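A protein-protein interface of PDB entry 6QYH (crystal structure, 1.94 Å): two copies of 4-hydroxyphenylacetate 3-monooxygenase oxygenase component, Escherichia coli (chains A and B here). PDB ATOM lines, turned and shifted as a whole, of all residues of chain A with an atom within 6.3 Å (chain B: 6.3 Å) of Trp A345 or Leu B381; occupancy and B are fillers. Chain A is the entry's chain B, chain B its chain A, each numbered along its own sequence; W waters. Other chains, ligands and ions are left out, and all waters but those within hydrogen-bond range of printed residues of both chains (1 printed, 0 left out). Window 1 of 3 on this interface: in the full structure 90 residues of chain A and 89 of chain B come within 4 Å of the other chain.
The side-chain amide nitrogen of Asn A347 lies close to the side-chain hydroxyl of Thr B377 (3.1 Å). SG of Cys B472 is in hydrogen-bond range of O of Gly A340, 3.6 Å away. The side-chain sulfur of Cys B472 sits at hydrogen-bond distance from the backbone NH of Ala A344 (3.7 Å). The side-chain carboxylate of Glu A341 lies close to the side-chain sulfur of Met B384, 3.7 Å away.
The indole nitrogen of Trp A345 sits at hydrogen-bond distance from the side-chain carboxylate of Glu A341 (3.0 Å). OE2 of Glu A341 is in salt-bridge range of NZ of Lys A388, 2.7 Å away. O of Val A343 sits close to OD1 of Asn A347 (3.5 Å). The backbone carbonyl oxygen (O) of Ala A344 lies within hydrogen-bond range of the side-chain hydroxyl (OG1) of Thr A348. The side-chain amide oxygen (OD1) of Asn A347 lies within hydrogen-bond range of the guanidinium group (NH1) of Arg A346, at 2.8 Å.
Ala A344 touches Thr B377 (O to CG2, 3.4 Å). Ala A344 touches Val B380 (CB to CG1, 3.7 Å). Trp B345 touches Trp A345 (CH2 to CH2, 3.8 Å). CH2 of Trp A345 touches CD2 of Leu B381, 3.9 Å away. Cys B472 touches Asn A347 (SG to ND2, 3.9 Å). Thr A348 touches Thr B377. Thr A348 touches Leu B381 (OG1 to CD1, 3.4 Å). CH2 of Trp B345 touches CD2 of Leu A381 (3.95 Å). Leu A381 touches Thr B348 (CD1 to OG1, 3.4 Å). SD of Met B384 touches NZ of Lys A388, at 3.8 Å.
Of chain A, only Trp A345 (3.9 Å) and Thr A348 (3.4 Å) come within 4 Å of Leu B381. Of the printed residues of chain A, Trp B345 touches Trp A345 and Leu A381. Printed residues of chain B within 4 Å of Val A343: Cys B472 (3.8 Å). Gln B376 touches none of the printed residues of chain A. The nearest printed residue of chain B that does not touch Trp A345 is Met B384 (4.4 Å). The nearest printed residue of chain A that does not touch Thr B348 is Thr A348 (4.3 Å).
Of the 18 printed residues of chain A, 9 touch a printed residue of chain B. Hydrophobic or aromatic side chains of chain B that line the printed part of chain A: Trp B345, Val B380, Leu B381 and Met B384. Among the printed residues, no Asp or Glu carboxylate lies within 4 Å of a Lys or Arg side-chain nitrogen of the other chain.
Trp A345 touches its own counterpart, Trp B345. Trp A345 touches Leu B381, and with the chains exchanged Leu A381 touches Trp B345. Thr A348 touches Leu B381, and with the chains exchanged Leu A381 touches Thr B348. Positions printed for both chains: 345, 348, 349, 381, 384 and 385.
Water W1 lies within hydrogen-bond range of O of Cys B472 (2.9 Å) and ND2 of Asn A347 (2.9 Å).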
ATOM      1  N   LEU A 313      21.128  -6.336  19.971  1.00  0.00           N
ATOM      2  CA  LEU A 313      21.089  -6.575  18.512  1.00  0.00           C
ATOM      3  C   LEU A 313      22.005  -7.736  18.091  1.00  0.00           C
ATOM      4  O   LEU A 313      21.621  -8.475  17.194  1.00  0.00           O
ATOM      5  CB  LEU A 313      21.336  -5.305  17.681  1.00  0.00           C
ATOM      6  CG  LEU A 313      20.301  -4.171  17.874  1.00  0.00           C
ATOM      7  CD1 LEU A 313      20.574  -3.030  16.936  1.00  0.00           C
ATOM      8  CD2 LEU A 313      18.836  -4.669  17.724  1.00  0.00           C
ATOM      9  N   GLY A 340      20.416  -9.739   6.288  1.00  0.00           N
ATOM     10  CA  GLY A 340      21.553  -8.853   6.008  1.00  0.00           C
ATOM     11  C   GLY A 340      21.309  -7.427   6.470  1.00  0.00           C
ATOM     12  O   GLY A 340      22.225  -6.775   6.976  1.00  0.00           O
ATOM     13  N   GLU A 341      20.059  -6.927   6.322  1.00  0.00           N
ATOM     14  CA  GLU A 341      19.741  -5.591   6.833  1.00  0.00           C
ATOM     15  C   GLU A 341      19.786  -5.521   8.375  1.00  0.00           C
ATOM     16  O   GLU A 341      20.297  -4.541   8.934  1.00  0.00           O
ATOM     17  CB  GLU A 341      18.405  -5.065   6.313  1.00  0.00           C
ATOM     18  CG  GLU A 341      18.251  -3.619   6.751  1.00  0.00           C
ATOM     19  CD  GLU A 341      17.060  -2.877   6.205  1.00  0.00           C
ATOM     20  OE1 GLU A 341      16.642  -3.192   5.070  1.00  0.00           O
ATOM     21  OE2 GLU A 341      16.567  -1.964   6.902  1.00  0.00           O
ATOM     22  N   VAL A 342      19.268  -6.562   9.059  1.00  0.00           N
ATOM     23  CA  VAL A 342      19.330  -6.643  10.529  1.00  0.00           C
ATOM     24  C   VAL A 342      20.817  -6.591  10.951  1.00  0.00           C
ATOM     25  O   VAL A 342      21.159  -5.874  11.897  1.00  0.00           O
ATOM     26  CB  VAL A 342      18.582  -7.894  11.086  1.00  0.00           C
ATOM     27  CG1 VAL A 342      18.791  -8.044  12.596  1.00  0.00           C
ATOM     28  CG2 VAL A 342      17.090  -7.836  10.733  1.00  0.00           C
ATOM     29  N   VAL A 343      21.686  -7.322  10.231  1.00  0.00           N
ATOM     30  CA  VAL A 343      23.140  -7.328  10.484  1.00  0.00           C
ATOM     31  C   VAL A 343      23.672  -5.880  10.361  1.00  0.00           C
ATOM     32  O   VAL A 343      24.435  -5.447  11.221  1.00  0.00           O
ATOM     33  CB  VAL A 343      23.925  -8.314   9.558  1.00  0.00           C
ATOM     34  CG1 VAL A 343      25.437  -8.132   9.702  1.00  0.00           C
ATOM     35  CG2 VAL A 343      23.529  -9.773   9.834  1.00  0.00           C
ATOM     36  N   ALA A 344      23.269  -5.142   9.296  1.00  0.00           N
ATOM     37  CA  ALA A 344      23.733  -3.769   9.074  1.00  0.00           C
ATOM     38  C   ALA A 344      23.346  -2.853  10.251  1.00  0.00           C
ATOM     39  O   ALA A 344      24.186  -2.084  10.705  1.00  0.00           O
ATOM     40  CB  ALA A 344      23.196  -3.213   7.742  1.00  0.00           C
ATOM     41  N   TRP A 345      22.103  -2.963  10.768  1.00  0.00           N
ATOM     42  CA  TRP A 345      21.661  -2.185  11.933  1.00  0.00           C
ATOM     43  C   TRP A 345      22.449  -2.545  13.193  1.00  0.00           C
ATOM     44  O   TRP A 345      22.899  -1.653  13.914  1.00  0.00           O
ATOM     45  CB  TRP A 345      20.159  -2.363  12.177  1.00  0.00           C
ATOM     46  CG  TRP A 345      19.312  -1.643  11.167  1.00  0.00           C
ATOM     47  CD1 TRP A 345      18.444  -2.200  10.275  1.00  0.00           C
ATOM     48  CD2 TRP A 345      19.276  -0.225  10.939  1.00  0.00           C
ATOM     49  NE1 TRP A 345      17.839  -1.209   9.520  1.00  0.00           N
ATOM     50  CE2 TRP A 345      18.333   0.012   9.914  1.00  0.00           C
ATOM     51  CE3 TRP A 345      19.945   0.877  11.517  1.00  0.00           C
ATOM     52  CZ2 TRP A 345      18.023   1.307   9.469  1.00  0.00           C
ATOM     53  CZ3 TRP A 345      19.630   2.159  11.080  1.00  0.00           C
ATOM     54  CH2 TRP A 345      18.697   2.364  10.059  1.00  0.00           C
ATOM     55  N   ARG A 346      22.662  -3.845  13.428  1.00  0.00           N
ATOM     56  CA  ARG A 346      23.465  -4.341  14.551  1.00  0.00           C
ATOM     57  C   ARG A 346      24.884  -3.692  14.461  1.00  0.00           C
ATOM     58  O   ARG A 346      25.392  -3.175  15.460  1.00  0.00           O
ATOM     59  CB  ARG A 346      23.512  -5.895  14.475  1.00  0.00           C
ATOM     60  CG  ARG A 346      24.539  -6.598  15.359  1.00  0.00           C
ATOM     61  CD  ARG A 346      25.890  -6.758  14.672  1.00  0.00           C
ATOM     62  NE  ARG A 346      26.863  -7.215  15.653  1.00  0.00           N
ATOM     63  CZ  ARG A 346      28.177  -7.076  15.573  1.00  0.00           C
ATOM     64  NH1 ARG A 346      28.726  -6.492  14.517  1.00  0.00           N
ATOM     65  NH2 ARG A 346      28.956  -7.523  16.548  1.00  0.00           N
ATOM     66  N   ASN A 347      25.504  -3.712  13.257  1.00  0.00           N
ATOM     67  CA  ASN A 347      26.842  -3.128  13.013  1.00  0.00           C
ATOM     68  C   ASN A 347      26.902  -1.628  13.291  1.00  0.00           C
ATOM     69  O   ASN A 347      27.913  -1.151  13.815  1.00  0.00           O
ATOM     70  CB  ASN A 347      27.313  -3.366  11.575  1.00  0.00           C
ATOM     71  CG  ASN A 347      27.592  -4.789  11.161  1.00  0.00           C
ATOM     72  OD1 ASN A 347      27.799  -5.689  11.979  1.00  0.00           O
ATOM     73  ND2 ASN A 347      27.593  -5.017   9.851  1.00  0.00           N
ATOM     74  N   THR A 348      25.824  -0.902  12.941  1.00  0.00           N
ATOM     75  CA  THR A 348      25.716   0.548  13.122  1.00  0.00           C
ATOM     76  C   THR A 348      25.927   0.977  14.572  1.00  0.00           C
ATOM     77  O   THR A 348      26.693   1.897  14.814  1.00  0.00           O
ATOM     78  CB  THR A 348      24.369   1.085  12.568  1.00  0.00           C
ATOM     79  OG1 THR A 348      24.221   0.675  11.209  1.00  0.00           O
ATOM     80  CG2 THR A 348      24.244   2.615  12.680  1.00  0.00           C
ATOM     81  N   PHE A 349      25.198   0.346  15.515  1.00  0.00           N
ATOM     82  CA  PHE A 349      25.257   0.720  16.927  1.00  0.00           C
ATOM     83  C   PHE A 349      26.640   0.425  17.524  1.00  0.00           C
ATOM     84  O   PHE A 349      27.148   1.236  18.305  1.00  0.00           O
ATOM     85  CB  PHE A 349      24.061   0.125  17.708  1.00  0.00           C
ATOM     86  CG  PHE A 349      22.796   0.800  17.193  1.00  0.00           C
ATOM     87  CD1 PHE A 349      21.960   0.148  16.289  1.00  0.00           C
ATOM     88  CD2 PHE A 349      22.536   2.139  17.479  1.00  0.00           C
ATOM     89  CE1 PHE A 349      20.839   0.803  15.738  1.00  0.00           C
ATOM     90  CE2 PHE A 349      21.411   2.784  16.955  1.00  0.00           C
ATOM     91  CZ  PHE A 349      20.569   2.116  16.085  1.00  0.00           C
ATOM     92  N   TRP A 350      27.306  -0.647  17.080  1.00  0.00           N
ATOM     93  CA  TRP A 350      28.690  -0.875  17.520  1.00  0.00           C
ATOM     94  C   TRP A 350      29.651   0.212  16.974  1.00  0.00           C
ATOM     95  O   TRP A 350      30.497   0.705  17.729  1.00  0.00           O
ATOM     96  CB  TRP A 350      29.179  -2.268  17.123  1.00  0.00           C
ATOM     97  CG  TRP A 350      28.589  -3.347  17.975  1.00  0.00           C
ATOM     98  CD1 TRP A 350      27.727  -4.326  17.581  1.00  0.00           C
ATOM     99  CD2 TRP A 350      28.831  -3.559  19.372  1.00  0.00           C
ATOM    100  NE1 TRP A 350      27.414  -5.136  18.644  1.00  0.00           N
ATOM    101  CE2 TRP A 350      28.098  -4.704  19.754  1.00  0.00           C
ATOM    102  CE3 TRP A 350      29.595  -2.885  20.346  1.00  0.00           C
ATOM    103  CZ2 TRP A 350      28.066  -5.172  21.078  1.00  0.00           C
ATOM    104  CZ3 TRP A 350      29.584  -3.366  21.654  1.00  0.00           C
ATOM    105  CH2 TRP A 350      28.822  -4.492  22.008  1.00  0.00           C
ATOM    106  N   LEU A 381      18.478   7.204  15.676  1.00  0.00           N
ATOM    107  CA  LEU A 381      18.434   5.958  14.907  1.00  0.00           C
ATOM    108  C   LEU A 381      17.780   4.766  15.603  1.00  0.00           C
ATOM    109  O   LEU A 381      17.133   3.974  14.914  1.00  0.00           O
ATOM    110  CB  LEU A 381      19.831   5.538  14.421  1.00  0.00           C
ATOM    111  CG  LEU A 381      20.605   6.467  13.446  1.00  0.00           C
ATOM    112  CD1 LEU A 381      21.889   5.790  12.989  1.00  0.00           C
ATOM    113  CD2 LEU A 381      19.771   6.877  12.232  1.00  0.00           C
ATOM    114  N   MET A 384      13.924   3.914  15.113  1.00  0.00           N
ATOM    115  CA  MET A 384      13.679   3.517  13.718  1.00  0.00           C
ATOM    116  C   MET A 384      14.243   2.131  13.434  1.00  0.00           C
ATOM    117  O   MET A 384      13.546   1.312  12.852  1.00  0.00           O
ATOM    118  CB  MET A 384      14.250   4.536  12.704  1.00  0.00           C
ATOM    119  CG  MET A 384      13.357   5.739  12.485  1.00  0.00           C
ATOM    120  SD  MET A 384      13.971   6.937  11.249  1.00  0.00           S
ATOM    121  CE  MET A 384      15.559   7.492  12.013  1.00  0.00           C
ATOM    122  N   ALA A 385      15.491   1.867  13.849  1.00  0.00           N
ATOM    123  CA  ALA A 385      16.126   0.565  13.654  1.00  0.00           C
ATOM    124  C   ALA A 385      15.364  -0.547  14.372  1.00  0.00           C
ATOM    125  O   ALA A 385      15.066  -1.560  13.759  1.00  0.00           O
ATOM    126  CB  ALA A 385      17.570   0.605  14.130  1.00  0.00           C
ATOM    127  N   LYS A 388      11.992  -1.316  12.724  1.00  0.00           N
ATOM    128  CA  LYS A 388      12.254  -1.959  11.433  1.00  0.00           C
ATOM    129  C   LYS A 388      12.703  -3.416  11.594  1.00  0.00           C
ATOM    130  O   LYS A 388      12.220  -4.296  10.881  1.00  0.00           O
ATOM    131  CB  LYS A 388      13.266  -1.122  10.602  1.00  0.00           C
ATOM    132  CG  LYS A 388      13.701  -1.734   9.270  1.00  0.00           C
ATOM    133  CD  LYS A 388      12.673  -1.557   8.158  1.00  0.00           C
ATOM    134  CE  LYS A 388      13.177  -2.035   6.805  1.00  0.00           C
ATOM    135  NZ  LYS A 388      14.098  -1.044   6.165  1.00  0.00           N
ATOM    136  N   ILE A 389      13.617  -3.672  12.551  1.00  0.00           N
ATOM    137  CA  ILE A 389      14.089  -5.026  12.827  1.00  0.00           C
ATOM    138  C   ILE A 389      12.893  -5.906  13.278  1.00  0.00           C
ATOM    139  O   ILE A 389      12.742  -7.015  12.781  1.00  0.00           O
ATOM    140  CB  ILE A 389      15.227  -4.999  13.878  1.00  0.00           C
ATOM    141  CG1 ILE A 389      16.533  -4.396  13.234  1.00  0.00           C
ATOM    142  CG2 ILE A 389      15.453  -6.412  14.464  1.00  0.00           C
ATOM    143  CD1 ILE A 389      17.573  -3.921  14.271  1.00  0.00           C
ATOM    144  N   ILE A 392      10.864  -6.765  10.226  1.00  0.00           N
ATOM    145  CA  ILE A 392      11.603  -7.761   9.427  1.00  0.00           C
ATOM    146  C   ILE A 392      11.369  -9.175  10.009  1.00  0.00           C
ATOM    147  O   ILE A 392      11.056 -10.100   9.253  1.00  0.00           O
ATOM    148  CB  ILE A 392      13.124  -7.408   9.309  1.00  0.00           C
ATOM    149  CG1 ILE A 392      13.326  -6.213   8.340  1.00  0.00           C
ATOM    150  CG2 ILE A 392      13.961  -8.642   8.875  1.00  0.00           C
ATOM    151  CD1 ILE A 392      14.807  -5.576   8.361  1.00  0.00           C
ATOM    152  N   TRP B 345      21.630  11.482  10.080  1.00  0.00           N
ATOM    153  CA  TRP B 345      22.177  10.713   8.959  1.00  0.00           C
ATOM    154  C   TRP B 345      23.573  11.192   8.568  1.00  0.00           C
ATOM    155  O   TRP B 345      24.475  10.372   8.380  1.00  0.00           O
ATOM    156  CB  TRP B 345      21.237  10.748   7.746  1.00  0.00           C
ATOM    157  CG  TRP B 345      20.001   9.911   7.935  1.00  0.00           C
ATOM    158  CD1 TRP B 345      18.709  10.349   7.975  1.00  0.00           C
ATOM    159  CD2 TRP B 345      19.953   8.489   8.143  1.00  0.00           C
ATOM    160  NE1 TRP B 345      17.852   9.280   8.155  1.00  0.00           N
ATOM    161  CE2 TRP B 345      18.593   8.127   8.247  1.00  0.00           C
ATOM    162  CE3 TRP B 345      20.930   7.482   8.206  1.00  0.00           C
ATOM    163  CZ2 TRP B 345      18.184   6.797   8.416  1.00  0.00           C
ATOM    164  CZ3 TRP B 345      20.521   6.164   8.346  1.00  0.00           C
ATOM    165  CH2 TRP B 345      19.164   5.835   8.468  1.00  0.00           C
ATOM    166  N   THR B 348      25.987   9.863  11.121  1.00  0.00           N
ATOM    167  CA  THR B 348      26.174   8.417  10.969  1.00  0.00           C
ATOM    168  C   THR B 348      27.349   8.062  10.063  1.00  0.00           C
ATOM    169  O   THR B 348      28.158   7.225  10.444  1.00  0.00           O
ATOM    170  CB  THR B 348      24.867   7.740  10.487  1.00  0.00           C
ATOM    171  OG1 THR B 348      23.811   8.095  11.383  1.00  0.00           O
ATOM    172  CG2 THR B 348      24.987   6.200  10.374  1.00  0.00           C
ATOM    173  N   PHE B 349      27.416   8.671   8.862  1.00  0.00           N
ATOM    174  CA  PHE B 349      28.442   8.353   7.876  1.00  0.00           C
ATOM    175  C   PHE B 349      29.827   8.797   8.356  1.00  0.00           C
ATOM    176  O   PHE B 349      30.800   8.071   8.142  1.00  0.00           O
ATOM    177  CB  PHE B 349      28.047   8.849   6.461  1.00  0.00           C
ATOM    178  CG  PHE B 349      26.843   8.032   6.000  1.00  0.00           C
ATOM    179  CD1 PHE B 349      26.992   6.704   5.593  1.00  0.00           C
ATOM    180  CD2 PHE B 349      25.554   8.557   6.067  1.00  0.00           C
ATOM    181  CE1 PHE B 349      25.880   5.924   5.268  1.00  0.00           C
ATOM    182  CE2 PHE B 349      24.435   7.777   5.734  1.00  0.00           C
ATOM    183  CZ  PHE B 349      24.599   6.462   5.344  1.00  0.00           C
ATOM    184  N   LEU B 352      30.721   6.051  10.996  1.00  0.00           N
ATOM    185  CA  LEU B 352      31.115   4.834  10.293  1.00  0.00           C
ATOM    186  C   LEU B 352      32.563   4.943   9.806  1.00  0.00           C
ATOM    187  O   LEU B 352      33.314   3.975   9.939  1.00  0.00           O
ATOM    188  CB  LEU B 352      30.186   4.533   9.095  1.00  0.00           C
ATOM    189  CG  LEU B 352      28.754   4.028   9.431  1.00  0.00           C
ATOM    190  CD1 LEU B 352      27.920   3.887   8.166  1.00  0.00           C
ATOM    191  CD2 LEU B 352      28.806   2.681  10.176  1.00  0.00           C
ATOM    192  N   GLN B 376      30.542  -2.612   4.847  1.00  0.00           N
ATOM    193  CA  GLN B 376      29.288  -3.245   4.419  1.00  0.00           C
ATOM    194  C   GLN B 376      28.084  -2.466   4.924  1.00  0.00           C
ATOM    195  O   GLN B 376      27.088  -2.369   4.214  1.00  0.00           O
ATOM    196  CB  GLN B 376      29.210  -4.704   4.917  1.00  0.00           C
ATOM    197  CG  GLN B 376      30.360  -5.600   4.455  1.00  0.00           C
ATOM    198  CD  GLN B 376      30.466  -5.700   2.949  1.00  0.00           C
ATOM    199  OE1 GLN B 376      29.610  -6.250   2.269  1.00  0.00           O
ATOM    200  NE2 GLN B 376      31.510  -5.157   2.394  1.00  0.00           N
ATOM    201  N   THR B 377      28.190  -1.893   6.136  1.00  0.00           N
ATOM    202  CA  THR B 377      27.111  -1.110   6.781  1.00  0.00           C
ATOM    203  C   THR B 377      26.887   0.163   6.002  1.00  0.00           C
ATOM    204  O   THR B 377      25.745   0.500   5.718  1.00  0.00           O
ATOM    205  CB  THR B 377      27.454  -0.842   8.256  1.00  0.00           C
ATOM    206  OG1 THR B 377      27.709  -2.095   8.870  1.00  0.00           O
ATOM    207  CG2 THR B 377      26.356  -0.118   8.998  1.00  0.00           C
ATOM    208  N   TYR B 378      27.980   0.867   5.642  1.00  0.00           N
ATOM    209  CA  TYR B 378      27.878   2.067   4.817  1.00  0.00           C
ATOM    210  C   TYR B 378      27.102   1.732   3.514  1.00  0.00           C
ATOM    211  O   TYR B 378      26.191   2.477   3.148  1.00  0.00           O
ATOM    212  CB  TYR B 378      29.280   2.690   4.502  1.00  0.00           C
ATOM    213  CG  TYR B 378      29.308   3.346   3.139  1.00  0.00           C
ATOM    214  CD1 TYR B 378      28.588   4.517   2.888  1.00  0.00           C
ATOM    215  CD2 TYR B 378      29.938   2.728   2.066  1.00  0.00           C
ATOM    216  CE1 TYR B 378      28.512   5.058   1.602  1.00  0.00           C
ATOM    217  CE2 TYR B 378      29.864   3.254   0.781  1.00  0.00           C
ATOM    218  CZ  TYR B 378      29.150   4.414   0.552  1.00  0.00           C
ATOM    219  OH  TYR B 378      29.096   4.922  -0.720  1.00  0.00           O
ATOM    220  N   ARG B 379      27.439   0.608   2.847  1.00  0.00           N
ATOM    221  CA  ARG B 379      26.789   0.222   1.580  1.00  0.00           C
ATOM    222  C   ARG B 379      25.292  -0.030   1.708  1.00  0.00           C
ATOM    223  O   ARG B 379      24.542   0.325   0.801  1.00  0.00           O
ATOM    224  CB  ARG B 379      27.483  -0.987   0.943  1.00  0.00           C
ATOM    225  CG  ARG B 379      28.931  -0.688   0.540  1.00  0.00           C
ATOM    226  CD  ARG B 379      29.644  -1.966   0.165  1.00  0.00           C
ATOM    227  NE  ARG B 379      29.140  -2.464  -1.110  1.00  0.00           N
ATOM    228  CZ  ARG B 379      29.024  -3.744  -1.434  1.00  0.00           C
ATOM    229  NH1 ARG B 379      29.388  -4.690  -0.575  1.00  0.00           N
ATOM    230  NH2 ARG B 379      28.557  -4.090  -2.625  1.00  0.00           N
ATOM    231  N   VAL B 380      24.855  -0.607   2.832  1.00  0.00           N
ATOM    232  CA  VAL B 380      23.426  -0.879   3.075  1.00  0.00           C
ATOM    233  C   VAL B 380      22.675   0.403   3.450  1.00  0.00           C
ATOM    234  O   VAL B 380      21.590   0.654   2.923  1.00  0.00           O
ATOM    235  CB  VAL B 380      23.222  -2.012   4.153  1.00  0.00           C
ATOM    236  CG1 VAL B 380      21.745  -2.172   4.532  1.00  0.00           C
ATOM    237  CG2 VAL B 380      23.797  -3.338   3.664  1.00  0.00           C
ATOM    238  N   LEU B 381      23.235   1.196   4.372  1.00  0.00           N
ATOM    239  CA  LEU B 381      22.553   2.398   4.867  1.00  0.00           C
ATOM    240  C   LEU B 381      22.470   3.556   3.879  1.00  0.00           C
ATOM    241  O   LEU B 381      21.483   4.269   3.909  1.00  0.00           O
ATOM    242  CB  LEU B 381      23.203   2.924   6.172  1.00  0.00           C
ATOM    243  CG  LEU B 381      23.191   2.047   7.440  1.00  0.00           C
ATOM    244  CD1 LEU B 381      23.759   2.830   8.635  1.00  0.00           C
ATOM    245  CD2 LEU B 381      21.776   1.487   7.777  1.00  0.00           C
ATOM    246  N   ALA B 382      23.532   3.801   3.077  1.00  0.00           N
ATOM    247  CA  ALA B 382      23.614   4.968   2.178  1.00  0.00           C
ATOM    248  C   ALA B 382      22.417   5.094   1.216  1.00  0.00           C
ATOM    249  O   ALA B 382      21.813   6.153   1.232  1.00  0.00           O
ATOM    250  CB  ALA B 382      24.943   4.986   1.424  1.00  0.00           C
ATOM    251  N   PRO B 383      21.955   4.032   0.483  1.00  0.00           N
ATOM    252  CA  PRO B 383      20.767   4.201  -0.388  1.00  0.00           C
ATOM    253  C   PRO B 383      19.504   4.614   0.384  1.00  0.00           C
ATOM    254  O   PRO B 383      18.772   5.477  -0.098  1.00  0.00           O
ATOM    255  CB  PRO B 383      20.608   2.810  -1.039  1.00  0.00           C
ATOM    256  CG  PRO B 383      21.984   2.219  -0.988  1.00  0.00           C
ATOM    257  CD  PRO B 383      22.527   2.673   0.327  1.00  0.00           C
ATOM    258  N   MET B 384      19.247   4.009   1.578  1.00  0.00           N
ATOM    259  CA  MET B 384      18.075   4.333   2.414  1.00  0.00           C
ATOM    260  C   MET B 384      18.172   5.764   2.957  1.00  0.00           C
ATOM    261  O   MET B 384      17.187   6.507   2.879  1.00  0.00           O
ATOM    262  CB  MET B 384      17.885   3.340   3.591  1.00  0.00           C
ATOM    263  CG  MET B 384      17.343   1.983   3.191  1.00  0.00           C
ATOM    264  SD  MET B 384      17.024   0.841   4.592  1.00  0.00           S
ATOM    265  CE  MET B 384      18.729   0.495   5.191  1.00  0.00           C
ATOM    266  N   ALA B 385      19.352   6.152   3.492  1.00  0.00           N
ATOM    267  CA  ALA B 385      19.573   7.508   4.025  1.00  0.00           C
ATOM    268  C   ALA B 385      19.390   8.553   2.941  1.00  0.00           C
ATOM    269  O   ALA B 385      18.639   9.488   3.159  1.00  0.00           O
ATOM    270  CB  ALA B 385      20.955   7.632   4.651  1.00  0.00           C
ATOM    271  N   TYR B 386      20.015   8.359   1.755  1.00  0.00           N
ATOM    272  CA  TYR B 386      19.949   9.316   0.667  1.00  0.00           C
ATOM    273  C   TYR B 386      18.528   9.518   0.153  1.00  0.00           C
ATOM    274  O   TYR B 386      18.097  10.664   0.037  1.00  0.00           O
ATOM    275  CB  TYR B 386      20.936   8.956  -0.458  1.00  0.00           C
ATOM    276  CG  TYR B 386      21.275  10.143  -1.331  1.00  0.00           C
ATOM    277  CD1 TYR B 386      22.309  11.017  -0.989  1.00  0.00           C
ATOM    278  CD2 TYR B 386      20.543  10.418  -2.483  1.00  0.00           C
ATOM    279  CE1 TYR B 386      22.625  12.115  -1.788  1.00  0.00           C
ATOM    280  CE2 TYR B 386      20.877  11.500  -3.311  1.00  0.00           C
ATOM    281  CZ  TYR B 386      21.921  12.341  -2.959  1.00  0.00           C
ATOM    282  OH  TYR B 386      22.283  13.402  -3.748  1.00  0.00           O
ATOM    283  N   ILE B 468      23.574  -5.857  -1.815  1.00  0.00           N
ATOM    284  CA  ILE B 468      24.337  -5.169  -0.751  1.00  0.00           C
ATOM    285  C   ILE B 468      24.021  -5.776   0.636  1.00  0.00           C
ATOM    286  O   ILE B 468      24.918  -5.907   1.473  1.00  0.00           O
ATOM    287  CB  ILE B 468      24.209  -3.615  -0.790  1.00  0.00           C
ATOM    288  CG1 ILE B 468      22.732  -3.147  -0.542  1.00  0.00           C
ATOM    289  CG2 ILE B 468      24.813  -3.035  -2.129  1.00  0.00           C
ATOM    290  CD1 ILE B 468      22.375  -1.678  -0.863  1.00  0.00           C
ATOM    291  N   CYS B 472      26.532  -7.969   3.214  1.00  0.00           N
ATOM    292  CA  CYS B 472      26.619  -7.578   4.616  1.00  0.00           C
ATOM    293  C   CYS B 472      26.455  -8.848   5.489  1.00  0.00           C
ATOM    294  O   CYS B 472      27.249  -9.072   6.402  1.00  0.00           O
ATOM    295  CB  CYS B 472      25.568  -6.513   4.938  1.00  0.00           C
ATOM    296  SG  CYS B 472      25.677  -5.866   6.619  1.00  0.00           S
HETATM  297  O   HOH W   1      28.517  -7.305   8.258  1.00  0.00           O
